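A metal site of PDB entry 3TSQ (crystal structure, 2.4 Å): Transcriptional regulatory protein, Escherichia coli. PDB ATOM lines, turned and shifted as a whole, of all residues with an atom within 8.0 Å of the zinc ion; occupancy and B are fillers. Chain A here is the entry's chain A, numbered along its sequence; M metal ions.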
ATOM      1  N   ARG A  33     -25.485 -29.571  16.833  1.00  0.00           N
ATOM      2  CA  ARG A  33     -24.475 -28.722  17.490  1.00  0.00           C
ATOM      3  C   ARG A  33     -23.227 -29.518  17.927  1.00  0.00           C
ATOM      4  O   ARG A  33     -22.080 -29.026  17.833  1.00  0.00           O
ATOM      5  CB  ARG A  33     -25.097 -27.982  18.680  1.00  0.00           C
ATOM      6  CG  ARG A  33     -24.351 -26.734  19.150  1.00  0.00           C
ATOM      7  CD  ARG A  33     -25.149 -25.929  20.270  1.00  0.00           C
ATOM      8  NE  ARG A  33     -25.069 -26.497  21.625  1.00  0.00           N
ATOM      9  CZ  ARG A  33     -25.974 -27.324  22.144  1.00  0.00           C
ATOM     10  NH1 ARG A  33     -27.029 -27.700  21.414  1.00  0.00           N
ATOM     11  NH2 ARG A  33     -25.847 -27.780  23.376  1.00  0.00           N
ATOM     12  N   ARG A  34     -23.436 -30.757  18.385  1.00  0.00           N
ATOM     13  CA  ARG A  34     -22.352 -31.650  18.786  1.00  0.00           C
ATOM     14  C   ARG A  34     -21.793 -32.549  17.674  1.00  0.00           C
ATOM     15  O   ARG A  34     -21.074 -33.514  17.954  1.00  0.00           O
ATOM     16  CB  ARG A  34     -22.801 -32.516  19.948  1.00  0.00           C
ATOM     17  CG  ARG A  34     -23.230 -31.717  21.149  1.00  0.00           C
ATOM     18  CD  ARG A  34     -23.105 -32.518  22.436  1.00  0.00           C
ATOM     19  NE  ARG A  34     -23.416 -31.634  23.545  1.00  0.00           N
ATOM     20  CZ  ARG A  34     -24.657 -31.365  23.927  1.00  0.00           C
ATOM     21  NH1 ARG A  34     -24.886 -30.509  24.949  1.00  0.00           N
ATOM     22  NH2 ARG A  34     -25.650 -31.932  23.274  1.00  0.00           N
ATOM     23  N   TYR A  37     -18.110 -33.498  17.610  1.00  0.00           N
ATOM     24  CA  TYR A  37     -17.494 -33.046  18.831  1.00  0.00           C
ATOM     25  C   TYR A  37     -16.973 -34.224  19.672  1.00  0.00           C
ATOM     26  O   TYR A  37     -17.764 -35.049  20.061  1.00  0.00           O
ATOM     27  CB  TYR A  37     -18.529 -32.248  19.622  1.00  0.00           C
ATOM     28  CG  TYR A  37     -17.928 -31.612  20.800  1.00  0.00           C
ATOM     29  CD1 TYR A  37     -16.790 -30.793  20.662  1.00  0.00           C
ATOM     30  CD2 TYR A  37     -18.436 -31.842  22.070  1.00  0.00           C
ATOM     31  CE1 TYR A  37     -16.202 -30.191  21.744  1.00  0.00           C
ATOM     32  CE2 TYR A  37     -17.877 -31.244  23.171  1.00  0.00           C
ATOM     33  CZ  TYR A  37     -16.761 -30.425  22.987  1.00  0.00           C
ATOM     34  OH  TYR A  37     -16.198 -29.847  24.053  1.00  0.00           O
ATOM     35  N   ARG A  59     -21.126 -31.043  38.798  1.00  0.00           N
ATOM     36  CA  ARG A  59     -20.177 -30.302  37.972  1.00  0.00           C
ATOM     37  C   ARG A  59     -19.155 -29.377  38.731  1.00  0.00           C
ATOM     38  O   ARG A  59     -17.957 -29.392  38.373  1.00  0.00           O
ATOM     39  CB  ARG A  59     -20.926 -29.550  36.858  1.00  0.00           C
ATOM     40  CG  ARG A  59     -20.056 -28.886  35.842  1.00  0.00           C
ATOM     41  CD  ARG A  59     -20.869 -28.161  34.799  1.00  0.00           C
ATOM     42  NE  ARG A  59     -20.029 -27.740  33.673  1.00  0.00           N
ATOM     43  CZ  ARG A  59     -19.950 -28.387  32.502  1.00  0.00           C
ATOM     44  NH1 ARG A  59     -20.656 -29.528  32.293  1.00  0.00           N
ATOM     45  NH2 ARG A  59     -19.132 -27.907  31.549  1.00  0.00           N
ATOM     46  N   PHE A  67     -15.179 -24.954  32.664  1.00  0.00           N
ATOM     47  CA  PHE A  67     -15.904 -24.693  31.427  1.00  0.00           C
ATOM     48  C   PHE A  67     -17.384 -24.313  31.690  1.00  0.00           C
ATOM     49  O   PHE A  67     -18.249 -25.182  31.685  1.00  0.00           O
ATOM     50  CB  PHE A  67     -15.858 -25.941  30.539  1.00  0.00           C
ATOM     51  CG  PHE A  67     -14.484 -26.403  30.163  1.00  0.00           C
ATOM     52  CD1 PHE A  67     -13.872 -25.945  29.028  1.00  0.00           C
ATOM     53  CD2 PHE A  67     -13.806 -27.350  30.948  1.00  0.00           C
ATOM     54  CE1 PHE A  67     -12.600 -26.370  28.670  1.00  0.00           C
ATOM     55  CE2 PHE A  67     -12.522 -27.793  30.596  1.00  0.00           C
ATOM     56  CZ  PHE A  67     -11.925 -27.311  29.462  1.00  0.00           C
ATOM     57  N   PRO A  68     -17.689 -23.015  31.933  1.00  0.00           N
ATOM     58  CA  PRO A  68     -19.139 -22.709  32.079  1.00  0.00           C
ATOM     59  C   PRO A  68     -19.968 -23.022  30.820  1.00  0.00           C
ATOM     60  O   PRO A  68     -19.499 -22.833  29.696  1.00  0.00           O
ATOM     61  CB  PRO A  68     -19.192 -21.226  32.459  1.00  0.00           C
ATOM     62  CG  PRO A  68     -17.813 -20.666  32.202  1.00  0.00           C
ATOM     63  CD  PRO A  68     -16.826 -21.834  32.103  1.00  0.00           C
ATOM     64  N   LEU A  69     -21.167 -23.561  31.034  1.00  0.00           N
ATOM     65  CA  LEU A  69     -22.012 -23.978  29.955  1.00  0.00           C
ATOM     66  C   LEU A  69     -22.542 -22.763  29.229  1.00  0.00           C
ATOM     67  O   LEU A  69     -22.981 -21.837  29.878  1.00  0.00           O
ATOM     68  CB  LEU A  69     -23.197 -24.800  30.463  1.00  0.00           C
ATOM     69  CG  LEU A  69     -22.894 -26.147  31.095  1.00  0.00           C
ATOM     70  CD1 LEU A  69     -24.143 -26.735  31.747  1.00  0.00           C
ATOM     71  CD2 LEU A  69     -22.336 -27.093  30.065  1.00  0.00           C
ATOM     72  N   CYS A  70     -22.515 -22.787  27.892  1.00  0.00           N
ATOM     73  CA  CYS A  70     -23.277 -21.871  27.067  1.00  0.00           C
ATOM     74  C   CYS A  70     -24.757 -22.172  27.380  1.00  0.00           C
ATOM     75  O   CYS A  70     -25.041 -23.186  28.014  1.00  0.00           O
ATOM     76  CB  CYS A  70     -22.978 -22.135  25.589  1.00  0.00           C
ATOM     77  SG  CYS A  70     -23.827 -23.642  24.958  1.00  0.00           S
ATOM     78  N   PRO A  71     -25.705 -21.302  26.932  1.00  0.00           N
ATOM     79  CA  PRO A  71     -27.111 -21.491  27.348  1.00  0.00           C
ATOM     80  C   PRO A  71     -27.847 -22.634  26.626  1.00  0.00           C
ATOM     81  O   PRO A  71     -28.834 -23.189  27.153  1.00  0.00           O
ATOM     82  CB  PRO A  71     -27.757 -20.122  27.011  1.00  0.00           C
ATOM     83  CG  PRO A  71     -26.574 -19.186  26.649  1.00  0.00           C
ATOM     84  CD  PRO A  71     -25.554 -20.114  26.077  1.00  0.00           C
ATOM     85  N   ALA A  72     -27.388 -22.976  25.431  1.00  0.00           N
ATOM     86  CA  ALA A  72     -28.006 -24.080  24.699  1.00  0.00           C
ATOM     87  C   ALA A  72     -27.793 -25.406  25.463  1.00  0.00           C
ATOM     88  O   ALA A  72     -28.720 -26.199  25.602  1.00  0.00           O
ATOM     89  CB  ALA A  72     -27.488 -24.133  23.283  1.00  0.00           C
ATOM     90  N   CYS A  73     -26.570 -25.594  25.974  1.00  0.00           N
ATOM     91  CA  CYS A  73     -26.222 -26.713  26.845  1.00  0.00           C
ATOM     92  C   CYS A  73     -26.879 -26.700  28.224  1.00  0.00           C
ATOM     93  O   CYS A  73     -27.187 -27.758  28.793  1.00  0.00           O
ATOM     94  CB  CYS A  73     -24.706 -26.736  27.032  1.00  0.00           C
ATOM     95  SG  CYS A  73     -23.840 -27.653  25.746  1.00  0.00           S
ATOM     96  N   ASP A  74     -27.069 -25.511  28.790  1.00  0.00           N
ATOM     97  CA  ASP A  74     -27.597 -25.369  30.138  1.00  0.00           C
ATOM     98  C   ASP A  74     -29.092 -25.690  30.217  1.00  0.00           C
ATOM     99  O   ASP A  74     -29.599 -26.184  31.241  1.00  0.00           O
ATOM    100  CB  ASP A  74     -27.307 -23.959  30.621  1.00  0.00           C
ATOM    101  CG  ASP A  74     -27.527 -23.787  32.096  1.00  0.00           C
ATOM    102  OD1 ASP A  74     -26.667 -24.205  32.912  1.00  0.00           O
ATOM    103  OD2 ASP A  74     -28.560 -23.192  32.436  1.00  0.00           O
ATOM    104  N   GLU A  76     -30.425 -27.993  28.271  1.00  0.00           N
ATOM    105  CA  GLU A  76     -30.421 -29.468  28.224  1.00  0.00           C
ATOM    106  C   GLU A  76     -30.123 -30.135  29.586  1.00  0.00           C
ATOM    107  O   GLU A  76     -30.870 -31.012  30.034  1.00  0.00           O
ATOM    108  CB  GLU A  76     -29.519 -30.002  27.092  1.00  0.00           C
ATOM    109  CG  GLU A  76     -30.088 -29.743  25.688  1.00  0.00           C
ATOM    110  CD  GLU A  76     -29.027 -29.602  24.562  1.00  0.00           C
ATOM    111  OE1 GLU A  76     -27.950 -30.238  24.627  1.00  0.00           O
ATOM    112  OE2 GLU A  76     -29.306 -28.848  23.581  1.00  0.00           O
ATOM    113  N   VAL A  90     -21.268 -32.666  30.678  1.00  0.00           N
ATOM    114  CA  VAL A  90     -21.789 -32.236  29.371  1.00  0.00           C
ATOM    115  C   VAL A  90     -21.091 -30.969  28.825  1.00  0.00           C
ATOM    116  O   VAL A  90     -20.698 -30.086  29.598  1.00  0.00           O
ATOM    117  CB  VAL A  90     -23.303 -31.974  29.481  1.00  0.00           C
ATOM    118  CG1 VAL A  90     -23.603 -30.774  30.384  1.00  0.00           C
ATOM    119  CG2 VAL A  90     -23.933 -31.753  28.076  1.00  0.00           C
ATOM    120  N   ALA A  91     -20.959 -30.888  27.498  1.00  0.00           N
ATOM    121  CA  ALA A  91     -20.417 -29.748  26.809  1.00  0.00           C
ATOM    122  C   ALA A  91     -20.763 -29.829  25.308  1.00  0.00           C
ATOM    123  O   ALA A  91     -21.297 -30.844  24.879  1.00  0.00           O
ATOM    124  CB  ALA A  91     -18.954 -29.704  27.002  1.00  0.00           C
ATOM    125  N   CYS A  92     -20.495 -28.752  24.559  1.00  0.00           N
ATOM    126  CA  CYS A  92     -20.556 -28.720  23.091  1.00  0.00           C
ATOM    127  C   CYS A  92     -19.358 -27.915  22.589  1.00  0.00           C
ATOM    128  O   CYS A  92     -18.610 -27.351  23.426  1.00  0.00           O
ATOM    129  CB  CYS A  92     -21.834 -28.078  22.574  1.00  0.00           C
ATOM    130  SG  CYS A  92     -21.851 -26.236  22.719  1.00  0.00           S
ATOM    131  N   PRO A  93     -19.157 -27.840  21.235  1.00  0.00           N
ATOM    132  CA  PRO A  93     -18.000 -27.085  20.736  1.00  0.00           C
ATOM    133  C   PRO A  93     -17.891 -25.655  21.268  1.00  0.00           C
ATOM    134  O   PRO A  93     -16.773 -25.173  21.447  1.00  0.00           O
ATOM    135  CB  PRO A  93     -18.192 -27.113  19.210  1.00  0.00           C
ATOM    136  CG  PRO A  93     -18.870 -28.409  18.967  1.00  0.00           C
ATOM    137  CD  PRO A  93     -19.895 -28.447  20.110  1.00  0.00           C
ATOM    138  N   GLU A  94     -19.033 -24.989  21.538  1.00  0.00           N
ATOM    139  CA  GLU A  94     -19.060 -23.598  22.047  1.00  0.00           C
ATOM    140  C   GLU A  94     -18.438 -23.426  23.433  1.00  0.00           C
ATOM    141  O   GLU A  94     -17.605 -22.531  23.638  1.00  0.00           O
ATOM    142  CB  GLU A  94     -20.505 -23.050  22.079  1.00  0.00           C
ATOM    143  CG  GLU A  94     -20.838 -22.022  20.964  1.00  0.00           C
ATOM    144  CD  GLU A  94     -20.151 -22.324  19.616  1.00  0.00           C
ATOM    145  OE1 GLU A  94     -19.582 -21.372  19.017  1.00  0.00           O
ATOM    146  OE2 GLU A  94     -20.175 -23.501  19.148  1.00  0.00           O
ATOM    147  N   CYS A  95     -18.806 -24.294  24.363  1.00  0.00           N
ATOM    148  CA  CYS A  95     -18.367 -24.134  25.756  1.00  0.00           C
ATOM    149  C   CYS A  95     -17.425 -25.202  26.266  1.00  0.00           C
ATOM    150  O   CYS A  95     -16.949 -25.085  27.380  1.00  0.00           O
ATOM    151  CB  CYS A  95     -19.578 -24.071  26.669  1.00  0.00           C
ATOM    152  SG  CYS A  95     -20.520 -25.571  26.603  1.00  0.00           S
ATOM    153  N   GLY A  96     -17.172 -26.258  25.494  1.00  0.00           N
ATOM    154  CA  GLY A  96     -16.419 -27.383  26.022  1.00  0.00           C
ATOM    155  C   GLY A  96     -14.914 -27.367  25.733  1.00  0.00           C
ATOM    156  O   GLY A  96     -14.384 -26.357  25.168  1.00  0.00           O
HETATM  157 ZN    ZN M   1     -22.299 -25.792  25.153  1.00  0.00          ZN
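The side-chain sulfur (SG) of Cys 73 sits close to the guanidinium group (NH2) of Arg 33 (3.1 Å). NE of Arg 33 sits close to SG of Cys 92, at 3.4 Å. SG of Cys 70 lies close to N of Ala 72, 3.7 Å away. The guanidinium group (NH1) of Arg 34 sits close to the side-chain sulfur (SG) of Cys 73 (3.1 Å). N of Glu 94 lies close to SG of Cys 92.
The zinc ion is bound by the side-chain sulfur (SG) of Cys 95, the side-chain sulfur (SG) of Cys 73, the side-chain sulfur (SG) of Cys 92 and the side-chain sulfur (SG) of Cys 70. The zinc ion has four donor atoms within binding distance.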
